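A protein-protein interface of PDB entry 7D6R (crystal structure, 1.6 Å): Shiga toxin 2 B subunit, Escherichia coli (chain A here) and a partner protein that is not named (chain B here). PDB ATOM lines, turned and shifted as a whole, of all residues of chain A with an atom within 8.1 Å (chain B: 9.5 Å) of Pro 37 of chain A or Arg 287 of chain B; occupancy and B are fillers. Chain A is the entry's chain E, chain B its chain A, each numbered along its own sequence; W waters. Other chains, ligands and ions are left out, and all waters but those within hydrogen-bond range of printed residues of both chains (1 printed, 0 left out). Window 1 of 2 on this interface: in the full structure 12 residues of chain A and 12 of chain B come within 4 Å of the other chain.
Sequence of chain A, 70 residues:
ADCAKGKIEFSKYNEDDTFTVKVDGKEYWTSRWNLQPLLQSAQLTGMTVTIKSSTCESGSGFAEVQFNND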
ATOM      1  N   PHE A  19      17.989  -8.468   5.054  1.00  0.00           N
ATOM      2  CA  PHE A  19      16.828  -8.167   5.890  1.00  0.00           C
ATOM      3  C   PHE A  19      16.343  -6.761   5.556  1.00  0.00           C
ATOM      4  O   PHE A  19      17.073  -5.789   5.757  1.00  0.00           O
ATOM      5  CB  PHE A  19      17.187  -8.283   7.372  1.00  0.00           C
ATOM      6  CG  PHE A  19      16.001  -8.286   8.297  1.00  0.00           C
ATOM      7  CD1 PHE A  19      15.290  -9.452   8.527  1.00  0.00           C
ATOM      8  CD2 PHE A  19      15.612  -7.118   8.968  1.00  0.00           C
ATOM      9  CE1 PHE A  19      14.201  -9.461   9.396  1.00  0.00           C
ATOM     10  CE2 PHE A  19      14.537  -7.127   9.835  1.00  0.00           C
ATOM     11  CZ  PHE A  19      13.824  -8.298  10.047  1.00  0.00           C
ATOM     12  N   ARG A  32      23.419  -7.467   8.336  1.00  0.00           N
ATOM     13  CA  ARG A  32      23.919  -7.732   9.680  1.00  0.00           C
ATOM     14  C   ARG A  32      22.860  -8.501  10.460  1.00  0.00           C
ATOM     15  O   ARG A  32      21.776  -7.962  10.724  1.00  0.00           O
ATOM     16  CB  ARG A  32      24.270  -6.434  10.406  1.00  0.00           C
ATOM     17  CG  ARG A  32      25.088  -5.426   9.593  1.00  0.00           C
ATOM     18  CD  ARG A  32      26.540  -5.841   9.421  1.00  0.00           C
ATOM     19  NE  ARG A  32      27.197  -4.992   8.427  1.00  0.00           N
ATOM     20  CZ  ARG A  32      27.968  -3.948   8.717  1.00  0.00           C
ATOM     21  NH1 ARG A  32      28.205  -3.621   9.979  1.00  0.00           N
ATOM     22  NH2 ARG A  32      28.510  -3.231   7.741  1.00  0.00           N
ATOM     23  N   TRP A  33      23.162  -9.752  10.835  1.00  0.00           N
ATOM     24  CA  TRP A  33      22.201 -10.518  11.628  1.00  0.00           C
ATOM     25  C   TRP A  33      21.958  -9.871  12.991  1.00  0.00           C
ATOM     26  O   TRP A  33      20.855  -9.998  13.543  1.00  0.00           O
ATOM     27  CB  TRP A  33      22.667 -11.970  11.799  1.00  0.00           C
ATOM     28  CG  TRP A  33      22.274 -12.902  10.666  1.00  0.00           C
ATOM     29  CD1 TRP A  33      22.080 -12.564   9.361  1.00  0.00           C
ATOM     30  CD2 TRP A  33      22.054 -14.323  10.750  1.00  0.00           C
ATOM     31  NE1 TRP A  33      21.739 -13.684   8.625  1.00  0.00           N
ATOM     32  CE2 TRP A  33      21.726 -14.773   9.455  1.00  0.00           C
ATOM     33  CE3 TRP A  33      22.095 -15.251  11.793  1.00  0.00           C
ATOM     34  CZ2 TRP A  33      21.437 -16.113   9.177  1.00  0.00           C
ATOM     35  CZ3 TRP A  33      21.821 -16.597  11.510  1.00  0.00           C
ATOM     36  CH2 TRP A  33      21.496 -17.006  10.214  1.00  0.00           C
ATOM     37  N   ASN A  34      22.962  -9.171  13.548  1.00  0.00           N
ATOM     38  CA  ASN A  34      22.760  -8.451  14.806  1.00  0.00           C
ATOM     39  C   ASN A  34      21.517  -7.572  14.741  1.00  0.00           C
ATOM     40  O   ASN A  34      20.799  -7.411  15.737  1.00  0.00           O
ATOM     41  CB  ASN A  34      23.966  -7.555  15.121  1.00  0.00           C
ATOM     42  CG  ASN A  34      25.124  -8.289  15.757  1.00  0.00           C
ATOM     43  OD1 ASN A  34      24.985  -9.383  16.295  1.00  0.00           O
ATOM     44  ND2 ASN A  34      26.294  -7.653  15.714  1.00  0.00           N
ATOM     45  N   LEU A  35      21.269  -6.964  13.579  1.00  0.00           N
ATOM     46  CA  LEU A  35      20.166  -6.021  13.455  1.00  0.00           C
ATOM     47  C   LEU A  35      18.812  -6.692  13.289  1.00  0.00           C
ATOM     48  O   LEU A  35      17.788  -6.009  13.443  1.00  0.00           O
ATOM     49  CB  LEU A  35      20.414  -5.065  12.283  1.00  0.00           C
ATOM     50  CG  LEU A  35      21.271  -3.846  12.624  1.00  0.00           C
ATOM     51  CD1 LEU A  35      21.672  -3.070  11.368  1.00  0.00           C
ATOM     52  CD2 LEU A  35      20.564  -2.911  13.600  1.00  0.00           C
ATOM     53  N   GLN A  36      18.752  -7.999  12.990  1.00  0.00           N
ATOM     54  CA  GLN A  36      17.433  -8.603  12.787  1.00  0.00           C
ATOM     55  C   GLN A  36      16.583  -8.595  14.053  1.00  0.00           C
ATOM     56  O   GLN A  36      15.446  -8.092  13.994  1.00  0.00           O
ATOM     57  CB  GLN A  36      17.562 -10.012  12.198  1.00  0.00           C
ATOM     58  CG  GLN A  36      18.174  -9.991  10.816  1.00  0.00           C
ATOM     59  CD  GLN A  36      18.049 -11.308  10.080  1.00  0.00           C
ATOM     60  OE1 GLN A  36      17.219 -12.162  10.424  1.00  0.00           O
ATOM     61  NE2 GLN A  36      18.864 -11.474   9.038  1.00  0.00           N
ATOM     62  N   PRO A  37      17.045  -9.091  15.208  1.00  0.00           N
ATOM     63  CA  PRO A  37      16.204  -8.991  16.408  1.00  0.00           C
ATOM     64  C   PRO A  37      15.987  -7.560  16.847  1.00  0.00           C
ATOM     65  O   PRO A  37      14.899  -7.249  17.347  1.00  0.00           O
ATOM     66  CB  PRO A  37      16.983  -9.784  17.470  1.00  0.00           C
ATOM     67  CG  PRO A  37      18.393  -9.842  16.948  1.00  0.00           C
ATOM     68  CD  PRO A  37      18.253  -9.900  15.465  1.00  0.00           C
ATOM     69  N   LEU A  38      16.988  -6.690  16.681  1.00  0.00           N
ATOM     70  CA  LEU A  38      16.832  -5.297  17.106  1.00  0.00           C
ATOM     71  C   LEU A  38      15.762  -4.598  16.281  1.00  0.00           C
ATOM     72  O   LEU A  38      14.895  -3.897  16.830  1.00  0.00           O
ATOM     73  CB  LEU A  38      18.168  -4.556  17.001  1.00  0.00           C
ATOM     74  CG  LEU A  38      19.331  -5.155  17.805  1.00  0.00           C
ATOM     75  CD1 LEU A  38      20.637  -4.415  17.527  1.00  0.00           C
ATOM     76  CD2 LEU A  38      19.049  -5.149  19.293  1.00  0.00           C
ATOM     77  N   LEU A  39      15.800  -4.779  14.958  1.00  0.00           N
ATOM     78  CA  LEU A  39      14.789  -4.165  14.099  1.00  0.00           C
ATOM     79  C   LEU A  39      13.415  -4.785  14.320  1.00  0.00           C
ATOM     80  O   LEU A  39      12.419  -4.064  14.427  1.00  0.00           O
ATOM     81  CB  LEU A  39      15.198  -4.272  12.625  1.00  0.00           C
ATOM     82  CG  LEU A  39      16.387  -3.385  12.223  1.00  0.00           C
ATOM     83  CD1 LEU A  39      16.974  -3.821  10.893  1.00  0.00           C
ATOM     84  CD2 LEU A  39      15.992  -1.901  12.157  1.00  0.00           C
ATOM     85  N   GLN A  40      13.324  -6.123  14.369  1.00  0.00           N
ATOM     86  CA  GLN A  40      12.001  -6.709  14.589  1.00  0.00           C
ATOM     87  C   GLN A  40      11.426  -6.284  15.935  1.00  0.00           C
ATOM     88  O   GLN A  40      10.230  -5.976  16.032  1.00  0.00           O
ATOM     89  CB  GLN A  40      12.024  -8.235  14.481  1.00  0.00           C
ATOM     90  CG  GLN A  40      10.589  -8.761  14.369  1.00  0.00           C
ATOM     91  CD  GLN A  40      10.407 -10.182  14.860  1.00  0.00           C
ATOM     92  OE1 GLN A  40      10.929 -10.564  15.907  1.00  0.00           O
ATOM     93  NE2 GLN A  40       9.632 -10.972  14.108  1.00  0.00           N
ATOM     94  N   SER A  41      12.257  -6.237  16.986  1.00  0.00           N
ATOM     95  CA  SER A  41      11.758  -5.726  18.264  1.00  0.00           C
ATOM     96  C   SER A  41      11.272  -4.291  18.109  1.00  0.00           C
ATOM     97  O   SER A  41      10.184  -3.937  18.598  1.00  0.00           O
ATOM     98  CB  SER A  41      12.832  -5.829  19.346  1.00  0.00           C
ATOM     99  OG  SER A  41      13.044  -7.190  19.721  1.00  0.00           O
ATOM    100  N   ALA A  42      12.041  -3.465  17.389  1.00  0.00           N
ATOM    101  CA  ALA A  42      11.601  -2.098  17.147  1.00  0.00           C
ATOM    102  C   ALA A  42      10.267  -2.085  16.417  1.00  0.00           C
ATOM    103  O   ALA A  42       9.385  -1.269  16.727  1.00  0.00           O
ATOM    104  CB  ALA A  42      12.664  -1.335  16.353  1.00  0.00           C
ATOM    105  N   GLN A  43      10.084  -3.010  15.468  1.00  0.00           N
ATOM    106  CA  GLN A  43       8.831  -3.066  14.731  1.00  0.00           C
ATOM    107  C   GLN A  43       7.669  -3.384  15.661  1.00  0.00           C
ATOM    108  O   GLN A  43       6.636  -2.700  15.635  1.00  0.00           O
ATOM    109  CB  GLN A  43       8.929  -4.104  13.605  1.00  0.00           C
ATOM    110  CG  GLN A  43       7.641  -4.231  12.784  1.00  0.00           C
ATOM    111  CD  GLN A  43       7.754  -5.319  11.719  1.00  0.00           C
ATOM    112  OE1 GLN A  43       8.843  -5.840  11.467  1.00  0.00           O
ATOM    113  NE2 GLN A  43       6.633  -5.655  11.087  1.00  0.00           N
ATOM    114  N   LEU A  44       7.832  -4.387  16.531  1.00  0.00           N
ATOM    115  CA  LEU A  44       6.652  -4.868  17.233  1.00  0.00           C
ATOM    116  C   LEU A  44       6.317  -4.015  18.445  1.00  0.00           C
ATOM    117  O   LEU A  44       5.199  -4.111  18.960  1.00  0.00           O
ATOM    118  CB  LEU A  44       6.823  -6.348  17.615  1.00  0.00           C
ATOM    119  CG  LEU A  44       7.887  -6.749  18.638  1.00  0.00           C
ATOM    120  CD1 LEU A  44       7.315  -6.749  20.041  1.00  0.00           C
ATOM    121  CD2 LEU A  44       8.418  -8.145  18.294  1.00  0.00           C
ATOM    122  N   PHE A  67      17.504   4.074  17.477  1.00  0.00           N
ATOM    123  CA  PHE A  67      16.251   3.582  18.042  1.00  0.00           C
ATOM    124  C   PHE A  67      15.774   4.525  19.136  1.00  0.00           C
ATOM    125  O   PHE A  67      16.518   4.796  20.085  1.00  0.00           O
ATOM    126  CB  PHE A  67      16.437   2.189  18.656  1.00  0.00           C
ATOM    127  CG  PHE A  67      16.907   1.139  17.688  1.00  0.00           C
ATOM    128  CD1 PHE A  67      18.263   0.928  17.475  1.00  0.00           C
ATOM    129  CD2 PHE A  67      15.993   0.353  17.007  1.00  0.00           C
ATOM    130  CE1 PHE A  67      18.700  -0.052  16.589  1.00  0.00           C
ATOM    131  CE2 PHE A  67      16.421  -0.627  16.119  1.00  0.00           C
ATOM    132  CZ  PHE A  67      17.773  -0.827  15.910  1.00  0.00           C
ATOM    133  N   ASN B 279       2.379 -10.546  25.887  1.00  0.00           N
ATOM    134  CA  ASN B 279       2.894 -11.075  24.618  1.00  0.00           C
ATOM    135  C   ASN B 279       3.966 -10.167  24.022  1.00  0.00           C
ATOM    136  O   ASN B 279       4.931 -10.645  23.408  1.00  0.00           O
ATOM    137  CB  ASN B 279       1.770 -11.248  23.594  1.00  0.00           C
ATOM    138  CG  ASN B 279       0.544 -11.914  24.153  1.00  0.00           C
ATOM    139  OD1 ASN B 279      -0.017 -11.478  25.157  1.00  0.00           O
ATOM    140  ND2 ASN B 279       0.083 -12.960  23.473  1.00  0.00           N
ATOM    141  N   THR B 280       3.809  -8.847  24.169  1.00  0.00           N
ATOM    142  CA  THR B 280       4.793  -7.913  23.628  1.00  0.00           C
ATOM    143  C   THR B 280       6.145  -8.085  24.318  1.00  0.00           C
ATOM    144  O   THR B 280       7.199  -8.207  23.664  1.00  0.00           O
ATOM    145  CB  THR B 280       4.273  -6.478  23.796  1.00  0.00           C
ATOM    146  OG1 THR B 280       3.061  -6.321  23.045  1.00  0.00           O
ATOM    147  CG2 THR B 280       5.296  -5.456  23.321  1.00  0.00           C
ATOM    148  N   ALA B 281       6.130  -8.071  25.655  1.00  0.00           N
ATOM    149  CA  ALA B 281       7.362  -8.292  26.402  1.00  0.00           C
ATOM    150  C   ALA B 281       7.979  -9.634  26.033  1.00  0.00           C
ATOM    151  O   ALA B 281       9.183  -9.717  25.765  1.00  0.00           O
ATOM    152  CB  ALA B 281       7.090  -8.203  27.907  1.00  0.00           C
ATOM    153  N   ALA B 282       7.157 -10.690  25.969  1.00  0.00           N
ATOM    154  CA  ALA B 282       7.693 -12.004  25.609  1.00  0.00           C
ATOM    155  C   ALA B 282       8.359 -11.976  24.240  1.00  0.00           C
ATOM    156  O   ALA B 282       9.348 -12.690  24.016  1.00  0.00           O
ATOM    157  CB  ALA B 282       6.576 -13.048  25.643  1.00  0.00           C
ATOM    158  N   ALA B 283       7.839 -11.160  23.320  1.00  0.00           N
ATOM    159  CA  ALA B 283       8.334 -11.129  21.946  1.00  0.00           C
ATOM    160  C   ALA B 283       9.629 -10.345  21.777  1.00  0.00           C
ATOM    161  O   ALA B 283      10.268 -10.469  20.717  1.00  0.00           O
ATOM    162  CB  ALA B 283       7.255 -10.556  21.014  1.00  0.00           C
ATOM    163  N   PHE B 284      10.036  -9.528  22.757  1.00  0.00           N
ATOM    164  CA  PHE B 284      11.401  -9.004  22.672  1.00  0.00           C
ATOM    165  C   PHE B 284      12.346  -9.572  23.727  1.00  0.00           C
ATOM    166  O   PHE B 284      13.541  -9.245  23.704  1.00  0.00           O
ATOM    167  CB  PHE B 284      11.424  -7.457  22.667  1.00  0.00           C
ATOM    168  CG  PHE B 284      10.936  -6.780  23.932  1.00  0.00           C
ATOM    169  CD1 PHE B 284      11.778  -6.587  25.021  1.00  0.00           C
ATOM    170  CD2 PHE B 284       9.671  -6.219  23.977  1.00  0.00           C
ATOM    171  CE1 PHE B 284      11.338  -5.916  26.165  1.00  0.00           C
ATOM    172  CE2 PHE B 284       9.223  -5.538  25.121  1.00  0.00           C
ATOM    173  CZ  PHE B 284      10.053  -5.393  26.212  1.00  0.00           C
ATOM    174  N   LEU B 285      11.865 -10.458  24.604  1.00  0.00           N
ATOM    175  CA  LEU B 285      12.700 -11.128  25.596  1.00  0.00           C
ATOM    176  C   LEU B 285      13.053 -12.556  25.206  1.00  0.00           C
ATOM    177  O   LEU B 285      13.703 -13.245  25.996  1.00  0.00           O
ATOM    178  CB  LEU B 285      12.016 -11.139  26.969  1.00  0.00           C
ATOM    179  CG  LEU B 285      11.742  -9.756  27.567  1.00  0.00           C
ATOM    180  CD1 LEU B 285      10.925  -9.877  28.847  1.00  0.00           C
ATOM    181  CD2 LEU B 285      13.024  -8.981  27.815  1.00  0.00           C
ATOM    182  N   ASN B 286      12.654 -13.016  24.018  1.00  0.00           N
ATOM    183  CA  ASN B 286      12.935 -14.373  23.558  1.00  0.00           C
ATOM    184  C   ASN B 286      14.191 -14.464  22.694  1.00  0.00           C
ATOM    185  O   ASN B 286      14.286 -15.344  21.834  1.00  0.00           O
ATOM    186  CB  ASN B 286      11.740 -14.938  22.783  1.00  0.00           C
ATOM    187  CG  ASN B 286      11.499 -14.199  21.479  1.00  0.00           C
ATOM    188  OD1 ASN B 286      12.071 -13.128  21.259  1.00  0.00           O
ATOM    189  ND2 ASN B 286      10.658 -14.761  20.606  1.00  0.00           N
ATOM    190  N   ARG B 287      15.151 -13.571  22.893  1.00  0.00           N
ATOM    191  CA  ARG B 287      16.394 -13.588  22.131  1.00  0.00           C
ATOM    192  C   ARG B 287      17.475 -14.315  22.925  1.00  0.00           C
ATOM    193  O   ARG B 287      17.581 -14.144  24.141  1.00  0.00           O
ATOM    194  CB  ARG B 287      16.842 -12.161  21.810  1.00  0.00           C
ATOM    195  CG  ARG B 287      16.151 -11.538  20.591  1.00  0.00           C
ATOM    196  CD  ARG B 287      14.697 -11.109  20.870  1.00  0.00           C
ATOM    197  NE  ARG B 287      14.182 -10.244  19.807  1.00  0.00           N
ATOM    198  CZ  ARG B 287      13.264 -10.591  18.901  1.00  0.00           C
ATOM    199  NH1 ARG B 287      12.728 -11.808  18.892  1.00  0.00           N
ATOM    200  NH2 ARG B 287      12.897  -9.714  17.981  1.00  0.00           N
ATOM    201  N   LYS B 288      18.273 -15.138  22.239  1.00  0.00           N
ATOM    202  CA  LYS B 288      19.409 -15.738  22.927  1.00  0.00           C
ATOM    203  C   LYS B 288      20.593 -14.773  22.881  1.00  0.00           C
ATOM    204  O   LYS B 288      20.494 -13.648  22.394  1.00  0.00           O
ATOM    205  CB  LYS B 288      19.776 -17.099  22.329  1.00  0.00           C
ATOM    206  CG  LYS B 288      20.511 -17.050  21.007  1.00  0.00           C
ATOM    207  CD  LYS B 288      20.755 -18.493  20.518  1.00  0.00           C
ATOM    208  CE  LYS B 288      21.384 -18.515  19.149  1.00  0.00           C
ATOM    209  NZ  LYS B 288      21.724 -19.905  18.718  1.00  0.00           N
ATOM    210  N   SER B 289      21.719 -15.210  23.437  1.00  0.00           N
ATOM    211  CA  SER B 289      22.928 -14.392  23.426  1.00  0.00           C
ATOM    212  C   SER B 289      23.268 -13.917  22.011  1.00  0.00           C
ATOM    213  O   SER B 289      23.314 -14.713  21.068  1.00  0.00           O
ATOM    214  CB  SER B 289      24.078 -15.208  24.016  1.00  0.00           C
ATOM    215  OG  SER B 289      25.297 -14.507  23.883  1.00  0.00           O
ATOM    216  N   GLN B 290      23.509 -12.605  21.870  1.00  0.00           N
ATOM    217  CA  GLN B 290      23.652 -11.992  20.546  1.00  0.00           C
ATOM    218  C   GLN B 290      24.840 -12.562  19.766  1.00  0.00           C
ATOM    219  O   GLN B 290      24.733 -12.814  18.559  1.00  0.00           O
ATOM    220  CB  GLN B 290      23.785 -10.473  20.695  1.00  0.00           C
ATOM    221  CG  GLN B 290      23.840  -9.676  19.370  1.00  0.00           C
ATOM    222  CD  GLN B 290      22.463  -9.418  18.789  1.00  0.00           C
ATOM    223  OE1 GLN B 290      21.599 -10.292  18.800  1.00  0.00           O
ATOM    224  NE2 GLN B 290      22.248  -8.205  18.284  1.00  0.00           N
ATOM    225  N   PHE B 291      25.988 -12.736  20.425  1.00  0.00           N
ATOM    226  CA  PHE B 291      27.141 -13.312  19.739  1.00  0.00           C
ATOM    227  C   PHE B 291      26.810 -14.686  19.174  1.00  0.00           C
ATOM    228  O   PHE B 291      27.183 -15.018  18.033  1.00  0.00           O
ATOM    229  CB  PHE B 291      28.329 -13.403  20.702  1.00  0.00           C
ATOM    230  CG  PHE B 291      29.628 -13.815  20.046  1.00  0.00           C
ATOM    231  CD1 PHE B 291      30.465 -12.863  19.492  1.00  0.00           C
ATOM    232  CD2 PHE B 291      30.010 -15.142  20.015  1.00  0.00           C
ATOM    233  CE1 PHE B 291      31.674 -13.233  18.906  1.00  0.00           C
ATOM    234  CE2 PHE B 291      31.224 -15.521  19.428  1.00  0.00           C
ATOM    235  CZ  PHE B 291      32.036 -14.563  18.865  1.00  0.00           C
ATOM    236  N   LEU B 292      26.088 -15.490  19.955  1.00  0.00           N
ATOM    237  CA  LEU B 292      25.742 -16.835  19.513  1.00  0.00           C
ATOM    238  C   LEU B 292      24.720 -16.796  18.389  1.00  0.00           C
ATOM    239  O   LEU B 292      24.761 -17.630  17.478  1.00  0.00           O
ATOM    240  CB  LEU B 292      25.224 -17.656  20.690  1.00  0.00           C
ATOM    241  CG  LEU B 292      26.184 -17.714  21.887  1.00  0.00           C
ATOM    242  CD1 LEU B 292      25.643 -18.618  22.974  1.00  0.00           C
ATOM    243  CD2 LEU B 292      27.575 -18.165  21.420  1.00  0.00           C
ATOM    244  N   TYR B 293      23.781 -15.849  18.450  1.00  0.00           N
ATOM    245  CA  TYR B 293      22.800 -15.711  17.383  1.00  0.00           C
ATOM    246  C   TYR B 293      23.470 -15.377  16.059  1.00  0.00           C
ATOM    247  O   TYR B 293      23.230 -16.040  15.035  1.00  0.00           O
ATOM    248  CB  TYR B 293      21.792 -14.635  17.772  1.00  0.00           C
ATOM    249  CG  TYR B 293      20.745 -14.328  16.722  1.00  0.00           C
ATOM    250  CD1 TYR B 293      19.644 -15.162  16.542  1.00  0.00           C
ATOM    251  CD2 TYR B 293      20.853 -13.189  15.930  1.00  0.00           C
ATOM    252  CE1 TYR B 293      18.678 -14.860  15.598  1.00  0.00           C
ATOM    253  CE2 TYR B 293      19.904 -12.891  14.980  1.00  0.00           C
ATOM    254  CZ  TYR B 293      18.811 -13.712  14.832  1.00  0.00           C
ATOM    255  OH  TYR B 293      17.854 -13.388  13.886  1.00  0.00           O
ATOM    256  N   THR B 294      24.348 -14.375  16.068  1.00  0.00           N
ATOM    257  CA  THR B 294      24.909 -13.884  14.824  1.00  0.00           C
ATOM    258  C   THR B 294      25.959 -14.828  14.247  1.00  0.00           C
ATOM    259  O   THR B 294      26.037 -14.968  13.017  1.00  0.00           O
ATOM    260  CB  THR B 294      25.458 -12.481  15.054  1.00  0.00           C
ATOM    261  OG1 THR B 294      24.347 -11.619  15.328  1.00  0.00           O
ATOM    262  CG2 THR B 294      26.211 -11.971  13.822  1.00  0.00           C
HETATM  263  O   HOH W   1      15.637  -7.513  20.719  1.00  0.00           O
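The guanidinium group of Arg 287 of chain B is in hydrogen-bond range of the backbone carbonyl oxygen of Pro 37 of chain A (3.2 Å). The side-chain amide oxygen (OE1) of Gln 40 of chain A lies within hydrogen-bond range of the guanidinium group (NH2) of Arg 287 of chain B. The side-chain hydroxyl (OG) of Ser 41 of chain A lies within hydrogen-bond range of the guanidinium group (NH2) of Arg 287 of chain B, 3.1 Å away. The side-chain amide nitrogen of Gln 290 of chain B lies within hydrogen-bond range of the backbone carbonyl oxygen of Asn 34 of chain A (3.0 Å). The side-chain hydroxyl (OG1) of Thr 294 of chain B lies within hydrogen-bond range of the side-chain amide oxygen (OD1) of Asn 34 of chain A.
The backbone carbonyl oxygen (O) of Ala 283 of chain B sits close to the side-chain amide oxygen (OD1) of Asn 286 of chain B, 3.3 Å away. The backbone carbonyl oxygen (O) of Ala 283 of chain B lies within hydrogen-bond range of the guanidinium group (NH1) of Arg 287 of chain B (3.3 Å). NH1 of Arg 287 of chain B lies within hydrogen-bond range of OD1 of Asn 286 of chain B. The side-chain hydroxyl (OG1) of Thr 294 of chain B lies within hydrogen-bond range of the backbone carbonyl oxygen (O) of Gln 290 of chain B, at 3.5 Å. The backbone carbonyl oxygen (O) of Pro 37 of chain A is in hydrogen-bond range of the side-chain hydroxyl (OG) of Ser 41 of chain A (3.0 Å).
Among the printed residues, pairs that only touch across the chains: Trp 33 of chain A with Tyr 293 of chain B (3.4 Å), Trp 33 of chain A with Thr 294 of chain B (3.8 Å), Gln 36 of chain A with Tyr 293 of chain B (3.7 Å), Pro 37 of chain A with Gln 290 of chain B (3.7 Å), Pro 37 of chain A with Tyr 293 of chain B (3.5 Å), Ser 41 of chain A with Phe 284 of chain B (3.4 Å), Leu 44 of chain A with Thr 280 of chain B (3.9 Å) and Leu 44 of chain A with Ala 283 of chain B (3.8 Å).
Of the printed residues of chain B, Asn 34 of chain A touches Gln 290 and Thr 294. Pro 37 of chain A touches just these residues of chain B: Arg 287 (3.2 Å), Gln 290 (3.7 Å) and Tyr 293 (3.5 Å). Gln 40 of chain A touches just one residue of chain B: Arg 287. Printed residues of chain B within 4 Å of Leu 44 of chain A: Thr 280 (3.9 Å) and Ala 283 (3.8 Å). Phe 67 of chain A touches none of the printed residues of chain B. Of the printed residues of chain A, Phe 284 of chain B touches Ser 41. No residue of chain A comes within 4 Å of Asn 286 of chain B. Arg 287 of chain B touches just these residues of chain A: Pro 37, Gln 40 and Ser 41. The nearest printed residue of chain B that does not touch Pro 37 of chain A is Thr 294 of chain B (6.3 Å). The nearest residue of chain A that does not touch Arg 287 of chain B is Leu 44 of chain A (4.8 Å). The nearest printed residue of chain A that does not touch Phe 284 of chain B is Leu 44 of chain A (4.6 Å).
Hydrophobic or aromatic side chains of chain A within 4 Å of the printed part of chain B: Trp 33, Pro 37 and Leu 44. Hydrophobic or aromatic side chains of chain B within 4 Å of the printed part of chain A: Ala 283, Phe 284 and Tyr 293. Among the printed residues, no Asp or Glu carboxylate lies within 4 Å of a Lys or Arg side-chain nitrogen of the other chain.
Water W1 lies within hydrogen-bond range of OG of Ser 41 of chain A (2.8 Å), NE of Arg 287 of chain B (3.2 Å) and O of Pro 37 of chain A (3.5 Å).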
